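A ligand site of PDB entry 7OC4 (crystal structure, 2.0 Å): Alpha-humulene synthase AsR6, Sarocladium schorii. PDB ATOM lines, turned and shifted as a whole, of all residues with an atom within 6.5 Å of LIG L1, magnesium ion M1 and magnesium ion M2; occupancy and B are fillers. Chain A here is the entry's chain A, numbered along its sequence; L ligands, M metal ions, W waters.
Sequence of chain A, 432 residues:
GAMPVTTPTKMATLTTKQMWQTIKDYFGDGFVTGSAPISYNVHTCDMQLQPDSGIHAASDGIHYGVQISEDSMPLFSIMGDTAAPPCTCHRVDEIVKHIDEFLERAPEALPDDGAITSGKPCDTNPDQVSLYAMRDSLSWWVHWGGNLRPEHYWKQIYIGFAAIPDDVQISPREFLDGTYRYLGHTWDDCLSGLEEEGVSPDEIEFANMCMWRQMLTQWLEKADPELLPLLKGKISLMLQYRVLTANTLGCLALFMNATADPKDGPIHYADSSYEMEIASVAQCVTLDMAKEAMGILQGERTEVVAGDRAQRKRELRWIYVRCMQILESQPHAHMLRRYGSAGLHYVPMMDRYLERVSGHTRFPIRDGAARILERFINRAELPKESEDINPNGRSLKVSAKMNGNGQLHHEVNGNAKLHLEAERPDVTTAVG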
ATOM      1  N   TRP A 140      10.712  12.589  -1.421  1.00  0.00           N
ATOM      2  CA  TRP A 140      10.791  12.178  -2.818  1.00  0.00           C
ATOM      3  C   TRP A 140       9.690  12.839  -3.629  1.00  0.00           C
ATOM      4  O   TRP A 140       9.948  13.467  -4.670  1.00  0.00           O
ATOM      5  CB  TRP A 140      10.664  10.665  -2.950  1.00  0.00           C
ATOM      6  CG  TRP A 140      11.808   9.880  -2.461  1.00  0.00           C
ATOM      7  CD1 TRP A 140      13.133  10.155  -2.638  1.00  0.00           C
ATOM      8  CD2 TRP A 140      11.744   8.676  -1.701  1.00  0.00           C
ATOM      9  NE1 TRP A 140      13.899   9.187  -2.038  1.00  0.00           N
ATOM     10  CE2 TRP A 140      13.065   8.266  -1.455  1.00  0.00           C
ATOM     11  CE3 TRP A 140      10.693   7.905  -1.208  1.00  0.00           C
ATOM     12  CZ2 TRP A 140      13.359   7.117  -0.728  1.00  0.00           C
ATOM     13  CZ3 TRP A 140      10.989   6.763  -0.493  1.00  0.00           C
ATOM     14  CH2 TRP A 140      12.310   6.382  -0.255  1.00  0.00           C
ATOM     15  N   ASP A 166      11.927  -1.566   2.126  1.00  0.00           N
ATOM     16  CA  ASP A 166      13.381  -1.433   2.048  1.00  0.00           C
ATOM     17  C   ASP A 166      14.011  -1.449   3.439  1.00  0.00           C
ATOM     18  O   ASP A 166      15.133  -1.928   3.601  1.00  0.00           O
ATOM     19  CB  ASP A 166      13.759  -0.150   1.310  1.00  0.00           C
ATOM     20  CG  ASP A 166      15.148  -0.231   0.668  1.00  0.00           C
ATOM     21  OD1 ASP A 166      15.297  -0.987  -0.319  1.00  0.00           O
ATOM     22  OD2 ASP A 166      16.075   0.457   1.135  1.00  0.00           O
ATOM     23  N   ASP A 167      13.281  -0.966   4.442  1.00  0.00           N
ATOM     24  CA  ASP A 167      13.809  -0.804   5.791  1.00  0.00           C
ATOM     25  C   ASP A 167      13.228  -1.788   6.801  1.00  0.00           C
ATOM     26  O   ASP A 167      13.682  -1.802   7.946  1.00  0.00           O
ATOM     27  CB  ASP A 167      13.554   0.637   6.283  1.00  0.00           C
ATOM     28  CG  ASP A 167      14.129   1.685   5.335  1.00  0.00           C
ATOM     29  OD1 ASP A 167      15.018   1.356   4.527  1.00  0.00           O
ATOM     30  OD2 ASP A 167      13.687   2.853   5.416  1.00  0.00           O
ATOM     31  N   GLN A 218      11.515  -7.271  -2.614  1.00  0.00           N
ATOM     32  CA  GLN A 218      12.164  -6.769  -1.403  1.00  0.00           C
ATOM     33  C   GLN A 218      12.361  -7.891  -0.392  1.00  0.00           C
ATOM     34  O   GLN A 218      13.402  -7.984   0.250  1.00  0.00           O
ATOM     35  CB  GLN A 218      11.324  -5.646  -0.791  1.00  0.00           C
ATOM     36  CG  GLN A 218      11.461  -4.291  -1.469  1.00  0.00           C
ATOM     37  CD  GLN A 218      12.711  -3.547  -1.050  1.00  0.00           C
ATOM     38  OE1 GLN A 218      13.601  -4.101  -0.410  1.00  0.00           O
ATOM     39  NE2 GLN A 218      12.784  -2.266  -1.409  1.00  0.00           N
ATOM     40  N   GLU A 221      15.060 -10.766  -1.649  1.00  0.00           N
ATOM     41  CA  GLU A 221      16.478 -10.450  -1.508  1.00  0.00           C
ATOM     42  C   GLU A 221      16.921 -10.419  -0.048  1.00  0.00           C
ATOM     43  O   GLU A 221      18.125 -10.476   0.215  1.00  0.00           O
ATOM     44  CB  GLU A 221      16.788  -9.113  -2.182  1.00  0.00           C
ATOM     45  CG  GLU A 221      16.259  -7.885  -1.481  1.00  0.00           C
ATOM     46  CD  GLU A 221      16.699  -6.601  -2.152  1.00  0.00           C
ATOM     47  OE1 GLU A 221      16.834  -6.594  -3.394  1.00  0.00           O
ATOM     48  OE2 GLU A 221      16.926  -5.600  -1.448  1.00  0.00           O
ATOM     49  N   LYS A 222      15.984 -10.328   0.901  1.00  0.00           N
ATOM     50  CA  LYS A 222      16.311 -10.446   2.306  1.00  0.00           C
ATOM     51  C   LYS A 222      16.268 -11.894   2.803  1.00  0.00           C
ATOM     52  O   LYS A 222      17.001 -12.237   3.743  1.00  0.00           O
ATOM     53  CB  LYS A 222      15.338  -9.619   3.155  1.00  0.00           C
ATOM     54  CG  LYS A 222      15.482  -8.118   3.010  1.00  0.00           C
ATOM     55  CD  LYS A 222      14.351  -7.403   3.730  1.00  0.00           C
ATOM     56  CE  LYS A 222      14.326  -5.924   3.392  1.00  0.00           C
ATOM     57  NZ  LYS A 222      14.021  -5.716   1.960  1.00  0.00           N
ATOM     58  N   ARG A 242      16.831  -4.111  -9.113  1.00  0.00           N
ATOM     59  CA  ARG A 242      16.763  -3.017  -8.155  1.00  0.00           C
ATOM     60  C   ARG A 242      15.659  -2.027  -8.509  1.00  0.00           C
ATOM     61  O   ARG A 242      15.140  -1.343  -7.616  1.00  0.00           O
ATOM     62  CB  ARG A 242      18.117  -2.300  -8.084  1.00  0.00           C
ATOM     63  CG  ARG A 242      18.467  -1.491  -9.328  1.00  0.00           C
ATOM     64  CD  ARG A 242      18.063  -0.022  -9.204  1.00  0.00           C
ATOM     65  NE  ARG A 242      18.884   0.704  -8.242  1.00  0.00           N
ATOM     66  CZ  ARG A 242      18.521   0.985  -7.003  1.00  0.00           C
ATOM     67  NH1 ARG A 242      17.342   0.598  -6.517  1.00  0.00           N
ATOM     68  NH2 ARG A 242      19.344   1.664  -6.217  1.00  0.00           N
ATOM     69  N   THR A 245      12.612  -3.463  -6.807  1.00  0.00           N
ATOM     70  CA  THR A 245      12.588  -3.258  -5.367  1.00  0.00           C
ATOM     71  C   THR A 245      12.341  -1.794  -5.010  1.00  0.00           C
ATOM     72  O   THR A 245      11.809  -1.501  -3.935  1.00  0.00           O
ATOM     73  CB  THR A 245      13.899  -3.724  -4.726  1.00  0.00           C
ATOM     74  OG1 THR A 245      14.994  -2.940  -5.221  1.00  0.00           O
ATOM     75  CG2 THR A 245      14.145  -5.188  -5.034  1.00  0.00           C
ATOM     76  N   ALA A 246      12.737  -0.872  -5.883  1.00  0.00           N
ATOM     77  CA  ALA A 246      12.442   0.532  -5.683  1.00  0.00           C
ATOM     78  C   ALA A 246      11.030   0.897  -6.116  1.00  0.00           C
ATOM     79  O   ALA A 246      10.472   1.884  -5.612  1.00  0.00           O
ATOM     80  CB  ALA A 246      13.448   1.402  -6.445  1.00  0.00           C
ATOM     81  N   CYS A 284      16.637   5.583 -10.676  1.00  0.00           N
ATOM     82  CA  CYS A 284      17.429   4.692  -9.829  1.00  0.00           C
ATOM     83  C   CYS A 284      18.917   4.851 -10.092  1.00  0.00           C
ATOM     84  O   CYS A 284      19.734   4.637  -9.189  1.00  0.00           O
ATOM     85  CB  CYS A 284      16.988   3.253 -10.034  1.00  0.00           C
ATOM     86  SG  CYS A 284      15.361   2.887  -9.324  1.00  0.00           S
ATOM     87  N   LEU A 287      19.907   8.041  -8.325  1.00  0.00           N
ATOM     88  CA  LEU A 287      19.927   7.728  -6.904  1.00  0.00           C
ATOM     89  C   LEU A 287      21.306   7.246  -6.477  1.00  0.00           C
ATOM     90  O   LEU A 287      21.886   7.751  -5.522  1.00  0.00           O
ATOM     91  CB  LEU A 287      18.852   6.671  -6.616  1.00  0.00           C
ATOM     92  CG  LEU A 287      18.896   5.938  -5.282  1.00  0.00           C
ATOM     93  CD1 LEU A 287      18.666   6.885  -4.119  1.00  0.00           C
ATOM     94  CD2 LEU A 287      17.863   4.814  -5.284  1.00  0.00           C
ATOM     95  N   ASP A 288      21.861   6.272  -7.206  1.00  0.00           N
ATOM     96  CA  ASP A 288      23.160   5.734  -6.832  1.00  0.00           C
ATOM     97  C   ASP A 288      24.304   6.637  -7.259  1.00  0.00           C
ATOM     98  O   ASP A 288      25.352   6.651  -6.595  1.00  0.00           O
ATOM     99  CB  ASP A 288      23.322   4.320  -7.404  1.00  0.00           C
ATOM    100  CG  ASP A 288      22.496   3.279  -6.651  1.00  0.00           C
ATOM    101  OD1 ASP A 288      22.133   3.517  -5.478  1.00  0.00           O
ATOM    102  OD2 ASP A 288      22.216   2.206  -7.222  1.00  0.00           O
ATOM    103  N   LYS A 291      24.351   9.089  -4.403  1.00  0.00           N
ATOM    104  CA  LYS A 291      24.835   8.392  -3.219  1.00  0.00           C
ATOM    105  C   LYS A 291      26.347   8.204  -3.270  1.00  0.00           C
ATOM    106  O   LYS A 291      27.034   8.350  -2.255  1.00  0.00           O
ATOM    107  CB  LYS A 291      24.126   7.039  -3.080  1.00  0.00           C
ATOM    108  CG  LYS A 291      22.756   7.131  -2.437  1.00  0.00           C
ATOM    109  CD  LYS A 291      21.855   5.991  -2.852  1.00  0.00           C
ATOM    110  CE  LYS A 291      22.331   4.654  -2.318  1.00  0.00           C
ATOM    111  NZ  LYS A 291      21.373   3.567  -2.677  1.00  0.00           N
ATOM    112  N   GLU A 300      26.954  -0.812   1.162  1.00  0.00           N
ATOM    113  CA  GLU A 300      25.597  -1.199   1.525  1.00  0.00           C
ATOM    114  C   GLU A 300      25.284  -2.575   0.944  1.00  0.00           C
ATOM    115  O   GLU A 300      25.805  -2.960  -0.112  1.00  0.00           O
ATOM    116  CB  GLU A 300      24.583  -0.151   1.061  1.00  0.00           C
ATOM    117  CG  GLU A 300      24.345  -0.069  -0.444  1.00  0.00           C
ATOM    118  CD  GLU A 300      23.248   0.920  -0.814  1.00  0.00           C
ATOM    119  OE1 GLU A 300      22.554   1.427   0.108  1.00  0.00           O
ATOM    120  OE2 GLU A 300      23.057   1.203  -2.020  1.00  0.00           O
ATOM    121  N   THR A 302      22.785  -3.957  -0.519  1.00  0.00           N
ATOM    122  CA  THR A 302      22.139  -4.018  -1.826  1.00  0.00           C
ATOM    123  C   THR A 302      22.866  -3.205  -2.883  1.00  0.00           C
ATOM    124  O   THR A 302      22.260  -2.820  -3.888  1.00  0.00           O
ATOM    125  CB  THR A 302      20.681  -3.533  -1.707  1.00  0.00           C
ATOM    126  OG1 THR A 302      20.667  -2.188  -1.206  1.00  0.00           O
ATOM    127  CG2 THR A 302      19.899  -4.435  -0.759  1.00  0.00           C
ATOM    128  N   VAL A 304      24.309  -1.779  -5.944  1.00  0.00           N
ATOM    129  CA  VAL A 304      24.111  -2.189  -7.328  1.00  0.00           C
ATOM    130  C   VAL A 304      25.438  -2.394  -8.043  1.00  0.00           C
ATOM    131  O   VAL A 304      25.548  -3.275  -8.903  1.00  0.00           O
ATOM    132  CB  VAL A 304      23.233  -1.147  -8.050  1.00  0.00           C
ATOM    133  CG1 VAL A 304      23.279  -1.334  -9.550  1.00  0.00           C
ATOM    134  CG2 VAL A 304      21.798  -1.235  -7.547  1.00  0.00           C
ATOM    135  N   TYR A 346      17.536  15.247  -4.802  1.00  0.00           N
ATOM    136  CA  TYR A 346      16.913  14.835  -3.552  1.00  0.00           C
ATOM    137  C   TYR A 346      17.855  14.029  -2.658  1.00  0.00           C
ATOM    138  O   TYR A 346      17.712  14.067  -1.440  1.00  0.00           O
ATOM    139  CB  TYR A 346      15.590  14.072  -3.795  1.00  0.00           C
ATOM    140  CG  TYR A 346      15.618  12.661  -4.374  1.00  0.00           C
ATOM    141  CD1 TYR A 346      16.282  11.625  -3.728  1.00  0.00           C
ATOM    142  CD2 TYR A 346      14.893  12.359  -5.519  1.00  0.00           C
ATOM    143  CE1 TYR A 346      16.266  10.336  -4.250  1.00  0.00           C
ATOM    144  CE2 TYR A 346      14.867  11.079  -6.045  1.00  0.00           C
ATOM    145  CZ  TYR A 346      15.555  10.075  -5.411  1.00  0.00           C
ATOM    146  OH  TYR A 346      15.531   8.802  -5.924  1.00  0.00           O
ATOM    147  N   ARG A 352      17.082  10.973   4.774  1.00  0.00           N
ATOM    148  CA  ARG A 352      17.333   9.556   4.577  1.00  0.00           C
ATOM    149  C   ARG A 352      18.801   9.288   4.266  1.00  0.00           C
ATOM    150  O   ARG A 352      19.389   8.327   4.780  1.00  0.00           O
ATOM    151  CB  ARG A 352      16.452   9.017   3.452  1.00  0.00           C
ATOM    152  CG  ARG A 352      16.589   7.521   3.210  1.00  0.00           C
ATOM    153  CD  ARG A 352      15.649   7.050   2.109  1.00  0.00           C
ATOM    154  NE  ARG A 352      15.757   5.610   1.871  1.00  0.00           N
ATOM    155  CZ  ARG A 352      15.176   4.689   2.612  1.00  0.00           C
ATOM    156  NH1 ARG A 352      14.449   5.005   3.673  1.00  0.00           N
ATOM    157  NH2 ARG A 352      15.326   3.401   2.295  1.00  0.00           N
ATOM    158  N   TYR A 353      19.405  10.135   3.450  1.00  0.00           N
ATOM    159  CA  TYR A 353      20.780   9.945   2.982  1.00  0.00           C
ATOM    160  C   TYR A 353      21.785  10.719   3.807  1.00  0.00           C
ATOM    161  O   TYR A 353      22.871  10.194   4.094  1.00  0.00           O
ATOM    162  CB  TYR A 353      20.855  10.349   1.511  1.00  0.00           C
ATOM    163  CG  TYR A 353      19.787   9.644   0.701  1.00  0.00           C
ATOM    164  CD1 TYR A 353      19.889   8.299   0.419  1.00  0.00           C
ATOM    165  CD2 TYR A 353      18.657  10.324   0.261  1.00  0.00           C
ATOM    166  CE1 TYR A 353      18.917   7.646  -0.289  1.00  0.00           C
ATOM    167  CE2 TYR A 353      17.674   9.680  -0.452  1.00  0.00           C
ATOM    168  CZ  TYR A 353      17.812   8.336  -0.720  1.00  0.00           C
ATOM    169  OH  TYR A 353      16.836   7.669  -1.429  1.00  0.00           O
ATOM    170  N   ARG A 356      22.765   8.715   6.695  1.00  0.00           N
ATOM    171  CA  ARG A 356      23.797   7.722   6.434  1.00  0.00           C
ATOM    172  C   ARG A 356      25.183   8.348   6.423  1.00  0.00           C
ATOM    173  O   ARG A 356      26.132   7.779   6.961  1.00  0.00           O
ATOM    174  CB  ARG A 356      23.514   7.025   5.100  1.00  0.00           C
ATOM    175  CG  ARG A 356      22.221   6.267   5.079  1.00  0.00           C
ATOM    176  CD  ARG A 356      21.952   5.668   3.714  1.00  0.00           C
ATOM    177  NE  ARG A 356      20.706   4.915   3.711  1.00  0.00           N
ATOM    178  CZ  ARG A 356      20.069   4.523   2.616  1.00  0.00           C
ATOM    179  NH1 ARG A 356      20.544   4.783   1.405  1.00  0.00           N
ATOM    180  NH2 ARG A 356      18.920   3.865   2.732  1.00  0.00           N
HETATM  181  P1  LIG L   1      17.723   3.846  -0.915  1.00  0.00           P
HETATM  182  O1  LIG L   1      17.359   3.150  -2.292  1.00  0.00           O
HETATM  183  P2  LIG L   1      17.462   1.651  -2.765  1.00  0.00           P
HETATM  184  S1  LIG L   1      16.208   1.577  -4.277  1.00  0.00           S
HETATM  185  O2  LIG L   1      17.575   2.737   0.130  1.00  0.00           O
HETATM  186  O3  LIG L   1      19.197   4.235  -1.029  1.00  0.00           O
HETATM  187  O4  LIG L   1      18.927   1.489  -3.336  1.00  0.00           O
HETATM  188  O5  LIG L   1      16.823   5.009  -0.668  1.00  0.00           O
HETATM  189  O6  LIG L   1      17.302   0.708  -1.639  1.00  0.00           O
HETATM  190  C1  LG2 L   2      10.584   5.295  -4.587  1.00  0.00           C
HETATM  191  C2  LG2 L   2      10.054   4.621  -3.338  1.00  0.00           C
HETATM  192  C3  LG2 L   2      13.746   4.030  -3.584  1.00  0.00           C
HETATM  193  C4  LG2 L   2      14.158   5.103  -4.242  1.00  0.00           C
HETATM  194  C5  LG2 L   2      13.692   5.391  -5.641  1.00  0.00           C
HETATM  195  C6  LG2 L   2      12.600   6.472  -5.592  1.00  0.00           C
HETATM  196  C7  LG2 L   2      14.094   3.613  -2.187  1.00  0.00           C
HETATM  197  C8  LG2 L   2      12.966   2.809  -1.468  1.00  0.00           C
HETATM  198  C9  LG2 L   2       9.901   4.916  -5.879  1.00  0.00           C
HETATM  199  C10 LG2 L   2      15.138   6.089  -3.684  1.00  0.00           C
HETATM  200  C11 LG2 L   2      12.959   1.375  -1.992  1.00  0.00           C
HETATM  201  C12 LG2 L   2      13.234   2.794   0.039  1.00  0.00           C
HETATM  202  C13 LG2 L   2      10.921   3.485  -2.863  1.00  0.00           C
HETATM  203  C14 LG2 L   2      11.666   3.511  -1.770  1.00  0.00           C
HETATM  204  C15 LG2 L   2      11.587   6.172  -4.528  1.00  0.00           C
HETATM  205 MG    MG M   1      16.634  -1.208  -1.728  1.00  0.00          MG
HETATM  206 MG    MG M   2      17.893   0.883   0.297  1.00  0.00          MG
HETATM  207  O   HOH W   1      18.785   0.720   2.265  1.00  0.00           O
HETATM  208  O   HOH W   2      17.921  -2.003  -3.127  1.00  0.00           O
HETATM  209  O   HOH W   3      18.091  -1.296  -0.166  1.00  0.00           O
HETATM  210  O   HOH W   4      15.313  -0.759  -3.231  1.00  0.00           O
HETATM  211  O   HOH W   5      19.897   0.950  -0.546  1.00  0.00           O
HETATM  212  O   HOH W   6      20.231  -0.607  -3.475  1.00  0.00           O
HETATM  213  O   HOH W   7      15.912  -3.121  -1.540  1.00  0.00           O
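O5 of LIG L1 sits at hydrogen-bond distance from OH of Tyr 353, 2.8 Å away. O3 of LIG L1 is in salt-bridge range of NZ of Lys 291. An oxygen (O4) of LIG L1 lies within salt-bridge range of the guanidinium group (NH2) of Arg 242 (2.9 Å). O5 of LIG L1 lies within salt-bridge range of NE of Arg 352. The guanidinium group of Arg 356 is in salt-bridge range of an oxygen (O3) of LIG L1 (2.8 Å).
The guanidinium group (NH1) of Arg 352 is in salt-bridge range of the side-chain carboxylate (OD2) of Asp 167, at 2.9 Å. The side-chain carboxylate (OD1) of Asp 166 sits close to the side-chain amide nitrogen (NE2) of Gln 218 (3.0 Å). OE2 of Glu 300 is in salt-bridge range of NZ of Lys 291 (3.0 Å). The side-chain carboxylate of Asp 166 lies close to the guanidinium group of Arg 352, at 3.3 Å. The side-chain amino group of Lys 291 lies within salt-bridge range of the side-chain carboxylate of Asp 288 (2.9 Å). The guanidinium group (NH2) of Arg 242 lies within salt-bridge range of the side-chain carboxylate (OD2) of Asp 288, 3.1 Å away. The side-chain hydroxyl (OH) of Tyr 353 is in hydrogen-bond range of the indole nitrogen (NE1) of Trp 140 (3.4 Å). The backbone carbonyl oxygen of Arg 242 sits at hydrogen-bond distance from the side-chain hydroxyl of Thr 245 (2.9 Å).
Ala 246 touches LIG L1. Leu 287 touches LIG L1.
Within 4 Å of magnesium ion M1: Asp 166. The nearest printed residue that does not touch magnesium ion M1 is Gln 218 (4.01 Å).
Merely in contact with magnesium ion M2: Arg 356 (3.98 Å).
Magnesium ion M1 is bound by OD1 of Asp 166, 2.0 Å away. An oxygen (O6) of LIG L1 is bound to magnesium ion M1 (2.0 Å). Water W4 is bound to magnesium ion M1, 2.1 Å away. Water W7 binds magnesium ion M1 (2.1 Å). Water W2 is bound to magnesium ion M1 (2.1 Å). Magnesium ion M1 is bound by water W3.
Magnesium ion M2 is bound by an oxygen (O2) of LIG L1 (1.9 Å), an oxygen (O6) of LIG L1 (2.0 Å), the side-chain carboxylate (OD2) of Asp 166 (2.0 Å), water W1 (2.2 Å), water W5 (2.2 Å) and water W3 (2.2 Å).
Water W7 bridges the side-chain carboxylate of Glu 221 and the side-chain amide oxygen of Gln 218. Water W4 lies within hydrogen-bond range of a sulfur (S1) of LIG L1 (2.7 Å), the side-chain hydroxyl of Thr 245 (3.0 Å) and the side-chain amide nitrogen of Gln 218 (3.5 Å). Water W5 lies within hydrogen-bond range of OE1 of Glu 300, O4 of LIG L1 and OG1 of Thr 302. Water W6 lies within hydrogen-bond range of an oxygen (O4) of LIG L1 (2.5 Å) and the side-chain hydroxyl of Thr 302 (2.8 Å).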
